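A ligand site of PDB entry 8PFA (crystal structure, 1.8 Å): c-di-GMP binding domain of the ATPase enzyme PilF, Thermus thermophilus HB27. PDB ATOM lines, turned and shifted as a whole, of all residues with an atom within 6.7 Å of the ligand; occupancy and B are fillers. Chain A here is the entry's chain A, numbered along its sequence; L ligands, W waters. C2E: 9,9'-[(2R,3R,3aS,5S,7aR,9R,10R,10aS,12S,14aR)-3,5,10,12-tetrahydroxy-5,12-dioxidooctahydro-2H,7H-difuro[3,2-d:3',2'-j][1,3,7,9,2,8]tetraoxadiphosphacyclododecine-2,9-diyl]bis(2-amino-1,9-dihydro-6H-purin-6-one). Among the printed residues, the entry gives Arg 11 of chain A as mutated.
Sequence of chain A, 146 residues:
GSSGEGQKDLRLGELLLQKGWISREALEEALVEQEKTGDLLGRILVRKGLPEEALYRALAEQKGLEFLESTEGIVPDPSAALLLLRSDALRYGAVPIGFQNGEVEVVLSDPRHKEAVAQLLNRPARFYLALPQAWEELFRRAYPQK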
ATOM      1  N   LEU A  10     -29.655 -31.451  -9.002  1.00  0.00           N
ATOM      2  CA  LEU A  10     -28.647 -30.472  -9.380  1.00  0.00           C
ATOM      3  C   LEU A  10     -28.251 -29.629  -8.176  1.00  0.00           C
ATOM      4  O   LEU A  10     -29.100 -29.230  -7.378  1.00  0.00           O
ATOM      5  CB  LEU A  10     -29.174 -29.569 -10.498  1.00  0.00           C
ATOM      6  CG  LEU A  10     -28.641 -29.853 -11.901  1.00  0.00           C
ATOM      7  CD1 LEU A  10     -29.140 -31.201 -12.397  1.00  0.00           C
ATOM      8  CD2 LEU A  10     -29.023 -28.736 -12.845  1.00  0.00           C
ATOM      9  N   ARG A  11     -26.961 -29.353  -8.072  1.00  0.00           N
ATOM     10  CA  ARG A  11     -26.479 -28.418  -7.062  1.00  0.00           C
ATOM     11  C   ARG A  11     -26.746 -26.974  -7.489  1.00  0.00           C
ATOM     12  O   ARG A  11     -26.990 -26.682  -8.657  1.00  0.00           O
ATOM     13  CB  ARG A  11     -24.987 -28.622  -6.800  1.00  0.00           C
ATOM     14  CG  ARG A  11     -24.614 -30.053  -6.494  1.00  0.00           C
ATOM     15  CD  ARG A  11     -23.414 -30.470  -7.303  1.00  0.00           C
ATOM     16  NE  ARG A  11     -22.188 -30.456  -6.499  1.00  0.00           N
ATOM     17  CZ  ARG A  11     -20.987 -30.710  -6.985  1.00  0.00           C
ATOM     18  NH1 ARG A  11     -19.925 -30.681  -6.185  1.00  0.00           N
ATOM     19  NH2 ARG A  11     -20.825 -30.976  -8.277  1.00  0.00           N
ATOM     20  N   LEU A  12     -26.661 -26.073  -6.510  1.00  0.00           N
ATOM     21  CA  LEU A  12     -27.019 -24.670  -6.750  1.00  0.00           C
ATOM     22  C   LEU A  12     -26.251 -24.094  -7.938  1.00  0.00           C
ATOM     23  O   LEU A  12     -26.831 -23.408  -8.791  1.00  0.00           O
ATOM     24  CB  LEU A  12     -26.736 -23.860  -5.509  1.00  0.00           C
ATOM     25  CG  LEU A  12     -26.834 -22.357  -5.764  1.00  0.00           C
ATOM     26  CD1 LEU A  12     -28.255 -21.968  -6.123  1.00  0.00           C
ATOM     27  CD2 LEU A  12     -26.340 -21.595  -4.556  1.00  0.00           C
ATOM     28  N   GLY A  13     -24.935 -24.322  -7.972  1.00  0.00           N
ATOM     29  CA  GLY A  13     -24.118 -23.739  -9.036  1.00  0.00           C
ATOM     30  C   GLY A  13     -24.550 -24.223 -10.404  1.00  0.00           C
ATOM     31  O   GLY A  13     -24.696 -23.416 -11.329  1.00  0.00           O
ATOM     32  N   GLU A  14     -24.807 -25.526 -10.539  1.00  0.00           N
ATOM     33  CA  GLU A  14     -25.252 -26.065 -11.815  1.00  0.00           C
ATOM     34  C   GLU A  14     -26.606 -25.506 -12.203  1.00  0.00           C
ATOM     35  O   GLU A  14     -26.859 -25.193 -13.372  1.00  0.00           O
ATOM     36  CB  GLU A  14     -25.303 -27.601 -11.750  1.00  0.00           C
ATOM     37  CD  GLU A  14     -24.000 -29.559 -10.756  1.00  0.00           C
ATOM     38  OE1 GLU A  14     -25.092 -29.897 -10.240  1.00  0.00           O
ATOM     39  OE2 GLU A  14     -22.957 -30.237 -10.619  1.00  0.00           O
ATOM     40  N   LEU A  15     -27.511 -25.380 -11.216  1.00  0.00           N
ATOM     41  CA  LEU A  15     -28.835 -24.811 -11.466  1.00  0.00           C
ATOM     42  C   LEU A  15     -28.714 -23.412 -12.061  1.00  0.00           C
ATOM     43  O   LEU A  15     -29.328 -23.119 -13.095  1.00  0.00           O
ATOM     44  CB  LEU A  15     -29.620 -24.773 -10.148  1.00  0.00           C
ATOM     45  CG  LEU A  15     -31.066 -25.266 -10.110  1.00  0.00           C
ATOM     46  CD1 LEU A  15     -31.257 -26.507 -10.936  1.00  0.00           C
ATOM     47  CD2 LEU A  15     -31.453 -25.544  -8.657  1.00  0.00           C
ATOM     48  N   LEU A  17     -26.128 -22.014 -13.537  1.00  0.00           N
ATOM     49  CA  LEU A  17     -25.502 -22.131 -14.850  1.00  0.00           C
ATOM     50  C   LEU A  17     -26.545 -22.493 -15.908  1.00  0.00           C
ATOM     51  O   LEU A  17     -26.579 -21.896 -16.996  1.00  0.00           O
ATOM     52  CB  LEU A  17     -24.402 -23.200 -14.804  1.00  0.00           C
ATOM     53  CG  LEU A  17     -22.957 -22.771 -14.669  1.00  0.00           C
ATOM     54  CD1 LEU A  17     -22.041 -23.992 -14.626  1.00  0.00           C
ATOM     55  CD2 LEU A  17     -22.562 -21.833 -15.801  1.00  0.00           C
ATOM     56  N   LEU A  27     -18.822 -18.855 -11.422  1.00  0.00           N
ATOM     57  CA  LEU A  27     -19.017 -19.998 -10.526  1.00  0.00           C
ATOM     58  C   LEU A  27     -17.696 -20.546 -10.022  1.00  0.00           C
ATOM     59  O   LEU A  27     -17.558 -20.876  -8.839  1.00  0.00           O
ATOM     60  CB  LEU A  27     -19.806 -21.094 -11.229  1.00  0.00           C
ATOM     61  CG  LEU A  27     -20.060 -22.361 -10.377  1.00  0.00           C
ATOM     62  CD1 LEU A  27     -20.708 -22.028  -9.035  1.00  0.00           C
ATOM     63  CD2 LEU A  27     -20.892 -23.378 -11.133  1.00  0.00           C
ATOM     64  N   LEU A  31     -16.406 -21.017  -6.180  1.00  0.00           N
ATOM     65  CA  LEU A  31     -16.054 -22.291  -5.580  1.00  0.00           C
ATOM     66  C   LEU A  31     -14.608 -22.303  -5.110  1.00  0.00           C
ATOM     67  O   LEU A  31     -14.277 -22.972  -4.122  1.00  0.00           O
ATOM     68  CB  LEU A  31     -16.329 -23.439  -6.560  1.00  0.00           C
ATOM     69  CG  LEU A  31     -17.803 -23.747  -6.842  1.00  0.00           C
ATOM     70  CD1 LEU A  31     -17.927 -24.727  -7.990  1.00  0.00           C
ATOM     71  CD2 LEU A  31     -18.484 -24.289  -5.607  1.00  0.00           C
ATOM     72  N   GLN A  34     -14.738 -20.473  -1.824  1.00  0.00           N
ATOM     73  CA  GLN A  34     -15.365 -21.306  -0.800  1.00  0.00           C
ATOM     74  C   GLN A  34     -14.382 -22.321  -0.239  1.00  0.00           C
ATOM     75  O   GLN A  34     -14.325 -22.521   0.975  1.00  0.00           O
ATOM     76  CB  GLN A  34     -16.602 -22.010  -1.357  1.00  0.00           C
ATOM     77  CG  GLN A  34     -17.337 -22.831  -0.308  1.00  0.00           C
ATOM     78  CD  GLN A  34     -18.570 -23.523  -0.847  1.00  0.00           C
ATOM     79  OE1 GLN A  34     -18.480 -24.410  -1.696  1.00  0.00           O
ATOM     80  NE2 GLN A  34     -19.730 -23.138  -0.329  1.00  0.00           N
ATOM     81  N   GLY A  38     -15.022 -21.500   3.192  1.00  0.00           N
ATOM     82  CA  GLY A  38     -16.151 -22.239   3.721  1.00  0.00           C
ATOM     83  C   GLY A  38     -17.450 -21.466   3.832  1.00  0.00           C
ATOM     84  O   GLY A  38     -18.400 -21.975   4.439  1.00  0.00           O
ATOM     85  N   ASP A  39     -17.532 -20.262   3.275  1.00  0.00           N
ATOM     86  CA  ASP A  39     -18.794 -19.533   3.253  1.00  0.00           C
ATOM     87  C   ASP A  39     -19.824 -20.261   2.391  1.00  0.00           C
ATOM     88  O   ASP A  39     -19.480 -21.021   1.477  1.00  0.00           O
ATOM     89  CB  ASP A  39     -18.583 -18.113   2.703  1.00  0.00           C
ATOM     90  CG  ASP A  39     -18.408 -17.069   3.790  1.00  0.00           C
ATOM     91  OD1 ASP A  39     -17.906 -17.413   4.883  1.00  0.00           O
ATOM     92  OD2 ASP A  39     -18.773 -15.891   3.561  1.00  0.00           O
ATOM     93  N   LEU A  40     -21.097 -20.000   2.676  1.00  0.00           N
ATOM     94  CA  LEU A  40     -22.180 -20.547   1.863  1.00  0.00           C
ATOM     95  C   LEU A  40     -22.033 -20.071   0.416  1.00  0.00           C
ATOM     96  O   LEU A  40     -21.685 -18.919   0.160  1.00  0.00           O
ATOM     97  CB  LEU A  40     -23.530 -20.088   2.397  1.00  0.00           C
ATOM     98  CG  LEU A  40     -24.513 -21.038   3.050  1.00  0.00           C
ATOM     99  CD1 LEU A  40     -25.818 -20.304   3.123  1.00  0.00           C
ATOM    100  CD2 LEU A  40     -24.660 -22.370   2.312  1.00  0.00           C
ATOM    101  N   LEU A  41     -22.294 -20.969  -0.539  1.00  0.00           N
ATOM    102  CA  LEU A  41     -21.996 -20.645  -1.933  1.00  0.00           C
ATOM    103  C   LEU A  41     -22.868 -19.507  -2.438  1.00  0.00           C
ATOM    104  O   LEU A  41     -22.377 -18.583  -3.102  1.00  0.00           O
ATOM    105  CB  LEU A  41     -22.188 -21.863  -2.831  1.00  0.00           C
ATOM    106  CG  LEU A  41     -21.732 -21.536  -4.261  1.00  0.00           C
ATOM    107  CD1 LEU A  41     -20.262 -21.195  -4.264  1.00  0.00           C
ATOM    108  CD2 LEU A  41     -22.022 -22.665  -5.235  1.00  0.00           C
ATOM    109  N   GLY A  42     -24.172 -19.558  -2.154  1.00  0.00           N
ATOM    110  CA  GLY A  42     -25.058 -18.499  -2.610  1.00  0.00           C
ATOM    111  C   GLY A  42     -24.654 -17.147  -2.069  1.00  0.00           C
ATOM    112  O   GLY A  42     -24.755 -16.137  -2.769  1.00  0.00           O
ATOM    113  N   ARG A  43     -24.162 -17.114  -0.829  1.00  0.00           N
ATOM    114  CA  ARG A  43     -23.699 -15.859  -0.241  1.00  0.00           C
ATOM    115  C   ARG A  43     -22.502 -15.292  -1.008  1.00  0.00           C
ATOM    116  O   ARG A  43     -22.414 -14.072  -1.213  1.00  0.00           O
ATOM    117  CB  ARG A  43     -23.339 -16.064   1.230  1.00  0.00           C
ATOM    118  CG  ARG A  43     -22.904 -14.801   1.950  1.00  0.00           C
ATOM    119  N   ILE A  44     -21.558 -16.148  -1.419  1.00  0.00           N
ATOM    120  CA  ILE A  44     -20.408 -15.672  -2.189  1.00  0.00           C
ATOM    121  C   ILE A  44     -20.860 -15.176  -3.552  1.00  0.00           C
ATOM    122  O   ILE A  44     -20.399 -14.133  -4.038  1.00  0.00           O
ATOM    123  CB  ILE A  44     -19.341 -16.766  -2.335  1.00  0.00           C
ATOM    124  CG1 ILE A  44     -18.902 -17.300  -0.965  1.00  0.00           C
ATOM    125  CG2 ILE A  44     -18.139 -16.240  -3.107  1.00  0.00           C
ATOM    126  CD1 ILE A  44     -18.017 -18.526  -1.046  1.00  0.00           C
ATOM    127  N   VAL A  46     -23.789 -13.995  -4.486  1.00  0.00           N
ATOM    128  CA  VAL A  46     -24.544 -12.740  -4.392  1.00  0.00           C
ATOM    129  C   VAL A  46     -23.602 -11.585  -4.080  1.00  0.00           C
ATOM    130  O   VAL A  46     -23.710 -10.496  -4.668  1.00  0.00           O
ATOM    131  CB  VAL A  46     -25.646 -12.862  -3.338  1.00  0.00           C
ATOM    132  CG1 VAL A  46     -26.191 -11.467  -2.987  1.00  0.00           C
ATOM    133  CG2 VAL A  46     -26.751 -13.739  -3.873  1.00  0.00           C
ATOM    134  N   LEU A  55     -30.736 -16.001  -6.788  1.00  0.00           N
ATOM    135  CA  LEU A  55     -30.358 -17.038  -5.855  1.00  0.00           C
ATOM    136  C   LEU A  55     -31.595 -17.711  -5.278  1.00  0.00           C
ATOM    137  O   LEU A  55     -31.673 -18.948  -5.219  1.00  0.00           O
ATOM    138  CB  LEU A  55     -29.497 -16.449  -4.731  1.00  0.00           C
ATOM    139  CG  LEU A  55     -29.235 -17.392  -3.562  1.00  0.00           C
ATOM    140  CD1 LEU A  55     -28.391 -18.593  -4.019  1.00  0.00           C
ATOM    141  CD2 LEU A  55     -28.545 -16.647  -2.417  1.00  0.00           C
ATOM    142  N   TYR A  56     -32.588 -16.933  -4.868  1.00  0.00           N
ATOM    143  CA  TYR A  56     -33.718 -17.553  -4.189  1.00  0.00           C
ATOM    144  C   TYR A  56     -34.588 -18.327  -5.158  1.00  0.00           C
ATOM    145  O   TYR A  56     -35.100 -19.397  -4.803  1.00  0.00           O
ATOM    146  CB  TYR A  56     -34.530 -16.513  -3.430  1.00  0.00           C
ATOM    147  CG  TYR A  56     -34.001 -16.335  -2.033  1.00  0.00           C
ATOM    148  CD1 TYR A  56     -32.784 -15.695  -1.804  1.00  0.00           C
ATOM    149  CD2 TYR A  56     -34.704 -16.815  -0.927  1.00  0.00           C
ATOM    150  CE1 TYR A  56     -32.285 -15.536  -0.532  1.00  0.00           C
ATOM    151  CE2 TYR A  56     -34.200 -16.656   0.362  1.00  0.00           C
ATOM    152  CZ  TYR A  56     -32.986 -16.026   0.548  1.00  0.00           C
ATOM    153  OH  TYR A  56     -32.464 -15.863   1.812  1.00  0.00           O
ATOM    154  N   LEU A  59     -32.782 -21.630  -5.487  1.00  0.00           N
ATOM    155  CA  LEU A  59     -32.929 -22.430  -4.271  1.00  0.00           C
ATOM    156  C   LEU A  59     -34.346 -22.987  -4.150  1.00  0.00           C
ATOM    157  O   LEU A  59     -34.549 -24.127  -3.710  1.00  0.00           O
ATOM    158  CB  LEU A  59     -32.556 -21.591  -3.059  1.00  0.00           C
ATOM    159  CG  LEU A  59     -31.042 -21.297  -2.915  1.00  0.00           C
ATOM    160  CD1 LEU A  59     -30.808 -20.309  -1.785  1.00  0.00           C
ATOM    161  CD2 LEU A  59     -30.221 -22.581  -2.690  1.00  0.00           C
ATOM    162  N   GLN A  62     -34.736 -25.933  -6.445  1.00  0.00           N
ATOM    163  CA  GLN A  62     -33.944 -27.075  -5.999  1.00  0.00           C
ATOM    164  C   GLN A  62     -34.678 -27.896  -4.950  1.00  0.00           C
ATOM    165  O   GLN A  62     -34.551 -29.133  -4.907  1.00  0.00           O
ATOM    166  CB  GLN A  62     -32.603 -26.585  -5.451  1.00  0.00           C
ATOM    167  CG  GLN A  62     -31.607 -27.673  -5.058  1.00  0.00           C
ATOM    168  CD  GLN A  62     -30.368 -27.097  -4.377  1.00  0.00           C
ATOM    169  OE1 GLN A  62     -30.472 -26.512  -3.301  1.00  0.00           O
ATOM    170  NE2 GLN A  62     -29.195 -27.290  -4.983  1.00  0.00           N
ATOM    171  N   LYS A  63     -35.444 -27.235  -4.088  1.00  0.00           N
ATOM    172  CA  LYS A  63     -36.163 -27.906  -3.010  1.00  0.00           C
ATOM    173  C   LYS A  63     -37.656 -28.023  -3.289  1.00  0.00           C
ATOM    174  O   LYS A  63     -38.430 -28.316  -2.384  1.00  0.00           O
ATOM    175  CB  LYS A  63     -35.914 -27.167  -1.695  1.00  0.00           C
ATOM    176  CG  LYS A  63     -34.575 -27.511  -1.023  1.00  0.00           C
ATOM    177  CD  LYS A  63     -34.599 -28.901  -0.394  1.00  0.00           C
ATOM    178  N   SER A 109     -38.275 -18.961   5.116  1.00  0.00           N
ATOM    179  CA  SER A 109     -37.236 -17.970   4.851  1.00  0.00           C
ATOM    180  C   SER A 109     -35.963 -18.586   4.277  1.00  0.00           C
ATOM    181  O   SER A 109     -35.158 -17.861   3.699  1.00  0.00           O
ATOM    182  CB  SER A 109     -36.881 -17.229   6.141  1.00  0.00           C
ATOM    183  OG  SER A 109     -36.173 -18.102   7.021  1.00  0.00           O
ATOM    184  N   ASP A 110     -35.790 -19.887   4.429  1.00  0.00           N
ATOM    185  CA  ASP A 110     -34.568 -20.606   4.073  1.00  0.00           C
ATOM    186  C   ASP A 110     -34.963 -22.005   3.629  1.00  0.00           C
ATOM    187  O   ASP A 110     -35.497 -22.800   4.428  1.00  0.00           O
ATOM    188  CB  ASP A 110     -33.606 -20.643   5.264  1.00  0.00           C
ATOM    189  CG  ASP A 110     -32.224 -21.199   4.920  1.00  0.00           C
ATOM    190  OD1 ASP A 110     -32.100 -21.958   3.935  1.00  0.00           O
ATOM    191  OD2 ASP A 110     -31.267 -20.889   5.654  1.00  0.00           O
ATOM    192  N   PRO A 111     -34.728 -22.350   2.361  1.00  0.00           N
ATOM    193  CA  PRO A 111     -35.095 -23.683   1.876  1.00  0.00           C
ATOM    194  C   PRO A 111     -34.398 -24.814   2.619  1.00  0.00           C
ATOM    195  O   PRO A 111     -34.921 -25.931   2.631  1.00  0.00           O
ATOM    196  CB  PRO A 111     -34.682 -23.657   0.402  1.00  0.00           C
ATOM    197  CG  PRO A 111     -33.657 -22.546   0.315  1.00  0.00           C
ATOM    198  CD  PRO A 111     -34.052 -21.532   1.332  1.00  0.00           C
ATOM    199  N   ARG A 112     -33.239 -24.563   3.224  1.00  0.00           N
ATOM    200  CA  ARG A 112     -32.574 -25.620   3.971  1.00  0.00           C
ATOM    201  C   ARG A 112     -33.388 -26.068   5.179  1.00  0.00           C
ATOM    202  O   ARG A 112     -33.092 -27.129   5.746  1.00  0.00           O
ATOM    203  CB  ARG A 112     -31.187 -25.166   4.446  1.00  0.00           C
ATOM    204  CG  ARG A 112     -30.183 -24.948   3.328  1.00  0.00           C
ATOM    205  CD  ARG A 112     -28.911 -24.334   3.903  1.00  0.00           C
ATOM    206  NE  ARG A 112     -29.166 -23.008   4.436  1.00  0.00           N
ATOM    207  CZ  ARG A 112     -28.288 -22.302   5.135  1.00  0.00           C
ATOM    208  NH1 ARG A 112     -27.078 -22.792   5.381  1.00  0.00           N
ATOM    209  NH2 ARG A 112     -28.625 -21.099   5.583  1.00  0.00           N
HETATM  210  P1  C2E L   1     -22.788 -25.088   0.376  1.00  0.00           P
HETATM  211  O2P C2E L   1     -22.256 -23.843  -0.291  1.00  0.00           O
HETATM  212  O1P C2E L   1     -22.419 -25.036   1.807  1.00  0.00           O
HETATM  213  O5' C2E L   1     -24.412 -25.145   0.415  1.00  0.00           O
HETATM  214  C5' C2E L   1     -25.060 -26.178   1.168  1.00  0.00           C
HETATM  215  C4' C2E L   1     -26.534 -26.161   0.617  1.00  0.00           C
HETATM  216  O4' C2E L   1     -27.103 -25.044   0.992  1.00  0.00           O
HETATM  217  C3' C2E L   1     -26.511 -26.164  -0.921  1.00  0.00           C
HETATM  218  O3' C2E L   1     -26.725 -27.445  -1.308  1.00  0.00           O
HETATM  219  C2' C2E L   1     -27.725 -25.291  -1.316  1.00  0.00           C
HETATM  220  O2' C2E L   1     -28.958 -26.140  -1.248  1.00  0.00           O
HETATM  221  C1' C2E L   1     -27.892 -24.519  -0.309  1.00  0.00           C
HETATM  222  N9  C2E L   1     -27.570 -23.109  -0.292  1.00  0.00           N
HETATM  223  C8  C2E L   1     -26.412 -22.939  -1.008  1.00  0.00           C
HETATM  224  N7  C2E L   1     -26.096 -21.585  -0.944  1.00  0.00           N
HETATM  225  C5  C2E L   1     -27.044 -20.984  -0.201  1.00  0.00           C
HETATM  226  C6  C2E L   1     -27.385 -19.571   0.288  1.00  0.00           C
HETATM  227  O6  C2E L   1     -26.693 -18.648   0.032  1.00  0.00           O
HETATM  228  N1  C2E L   1     -28.525 -19.356   1.111  1.00  0.00           N
HETATM  229  C2  C2E L   1     -29.395 -20.458   1.476  1.00  0.00           C
HETATM  230  N2  C2E L   1     -30.539 -20.299   2.284  1.00  0.00           N
HETATM  231  N3  C2E L   1     -29.096 -21.771   1.002  1.00  0.00           N
HETATM  232  C4  C2E L   1     -27.913 -21.959   0.179  1.00  0.00           C
HETATM  233  P11 C2E L   1     -26.164 -27.825  -2.899  1.00  0.00           P
HETATM  234  O21 C2E L   1     -26.769 -27.029  -4.047  1.00  0.00           O
HETATM  235  O11 C2E L   1     -26.572 -29.253  -3.108  1.00  0.00           O
HETATM  236  O5A C2E L   1     -24.434 -27.624  -2.768  1.00  0.00           O
HETATM  237  C5A C2E L   1     -23.762 -28.650  -2.034  1.00  0.00           C
HETATM  238  C4A C2E L   1     -22.329 -28.227  -2.097  1.00  0.00           C
HETATM  239  O4A C2E L   1     -21.833 -28.353  -3.292  1.00  0.00           O
HETATM  240  C3A C2E L   1     -22.229 -26.606  -1.732  1.00  0.00           C
HETATM  241  O3A C2E L   1     -22.091 -26.535  -0.226  1.00  0.00           O
HETATM  242  C2A C2E L   1     -21.236 -26.156  -2.333  1.00  0.00           C
HETATM  243  O2A C2E L   1     -19.969 -26.283  -1.504  1.00  0.00           O
HETATM  244  C1A C2E L   1     -21.095 -27.081  -3.654  1.00  0.00           C
HETATM  245  N91 C2E L   1     -21.698 -26.637  -4.737  1.00  0.00           N
HETATM  246  C81 C2E L   1     -22.880 -25.957  -4.924  1.00  0.00           C
HETATM  247  N71 C2E L   1     -23.060 -25.823  -6.266  1.00  0.00           N
HETATM  248  C51 C2E L   1     -22.015 -26.427  -6.876  1.00  0.00           C
HETATM  249  C61 C2E L   1     -21.656 -26.609  -8.359  1.00  0.00           C
HETATM  250  O61 C2E L   1     -22.344 -26.183  -9.193  1.00  0.00           O
HETATM  251  N11 C2E L   1     -20.448 -27.306  -8.733  1.00  0.00           N
HETATM  252  C21 C2E L   1     -19.581 -27.846  -7.705  1.00  0.00           C
HETATM  253  N21 C2E L   1     -18.333 -28.580  -8.083  1.00  0.00           N
HETATM  254  N31 C2E L   1     -19.926 -27.669  -6.289  1.00  0.00           N
HETATM  255  C41 C2E L   1     -21.175 -26.934  -5.911  1.00  0.00           C
HETATM  256  O   HOH W   1     -29.442 -17.156   2.339  1.00  0.00           O
HETATM  257  O   HOH W   2     -22.638 -27.855   3.384  1.00  0.00           O
HETATM  258  O   HOH W   3     -32.124 -17.985   3.328  1.00  0.00           O
HETATM  259  O   HOH W   4     -23.018 -24.516   4.853  1.00  0.00           O
HETATM  260  O   HOH W   5     -27.175 -16.043   1.098  1.00  0.00           O
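The backbone NH (N) of Leu 41 sits at hydrogen-bond distance from an oxygen (O2P) of the ligand (2.9 Å).
A nitrogen (N7) of the ligand is in hydrogen-bond range of the backbone NH (N) of Gly 42, at 3.0 Å.
The backbone NH of Arg 43 sits at hydrogen-bond distance from an oxygen (O6) of the ligand (3.1 Å).
An oxygen (O2') of the ligand sits at hydrogen-bond distance from the side-chain amide oxygen (OE1) of Gln 62 (2.6 Å).
An oxygen (O21) of the ligand is in hydrogen-bond range of the backbone NH of Leu 12, at 2.6 Å.
A nitrogen (N31) of the ligand is in hydrogen-bond range of the guanidinium group (NH1) of Arg 11 (3.0 Å).
The side-chain amide oxygen of Gln 34 sits at hydrogen-bond distance from an oxygen (O2A) of the ligand.
The backbone NH (N) of Gly 13 is in hydrogen-bond range of a nitrogen (N71) of the ligand (2.9 Å).
O61 of the ligand is in hydrogen-bond range of N of Glu 14 (2.9 Å).
The side-chain carboxylate (OD1) of Asp 110 sits at hydrogen-bond distance from a nitrogen (N2) of the ligand (2.8 Å).
OD2 of Asp 110 lies within salt-bridge range of NH2 of Arg 112, at 2.7 Å.
OE2 of Glu 14 lies within salt-bridge range of NH2 of Arg 11.
The side-chain amide nitrogen (NE2) of Gln 34 lies close to the backbone NH (N) of Leu 41 (3.4 Å).
The backbone NH of Leu 12 sits close to the side-chain amide nitrogen of Gln 62, 3.2 Å away.
The backbone carbonyl oxygen (O) of Leu 10 lies within hydrogen-bond range of the side-chain amide nitrogen (NE2) of Gln 62 (3.1 Å).
NE2 of Gln 34 lies within hydrogen-bond range of O of Asp 39.
Leu 27 touches the ligand.
Leu 31 touches the ligand (CD1 to C21, 3.5 Å).
Leu 40 touches the ligand.
CD2 of Leu 55 touches O6 of the ligand, at 3.7 Å.
Leu 59 touches the ligand.
Pro 111 touches the ligand (CD to N2, 3.8 Å).
Arg 112 touches the ligand.
Hydrophobic or aromatic side chains that line the ligand: Leu 12, Leu 27, Leu 31, Leu 40, Leu 41, Leu 55, Leu 59 and Pro 111.
17 residues have an atom within 4 Å of the ligand: Arg 11, Leu 12, Gly 13, Glu 14, Leu 27, Leu 31, Gln 34, Leu 40, Leu 41, Gly 42, Arg 43, Leu 55, Leu 59, Gln 62, Asp 110, Pro 111 and Arg 112.
The nearest printed residue that does not touch the ligand is Asp 39 (4.3 Å).
Water W1 bridges N1 of the ligand (2.7 Å) and OH of Tyr 56 (3.3 Å).
Water W3 lies within hydrogen-bond range of the side-chain hydroxyl (OH) of Tyr 56 (2.6 Å), a nitrogen (N2) of the ligand (3.0 Å) and the backbone carbonyl oxygen (O) of Ser 109 (3.1 Å).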
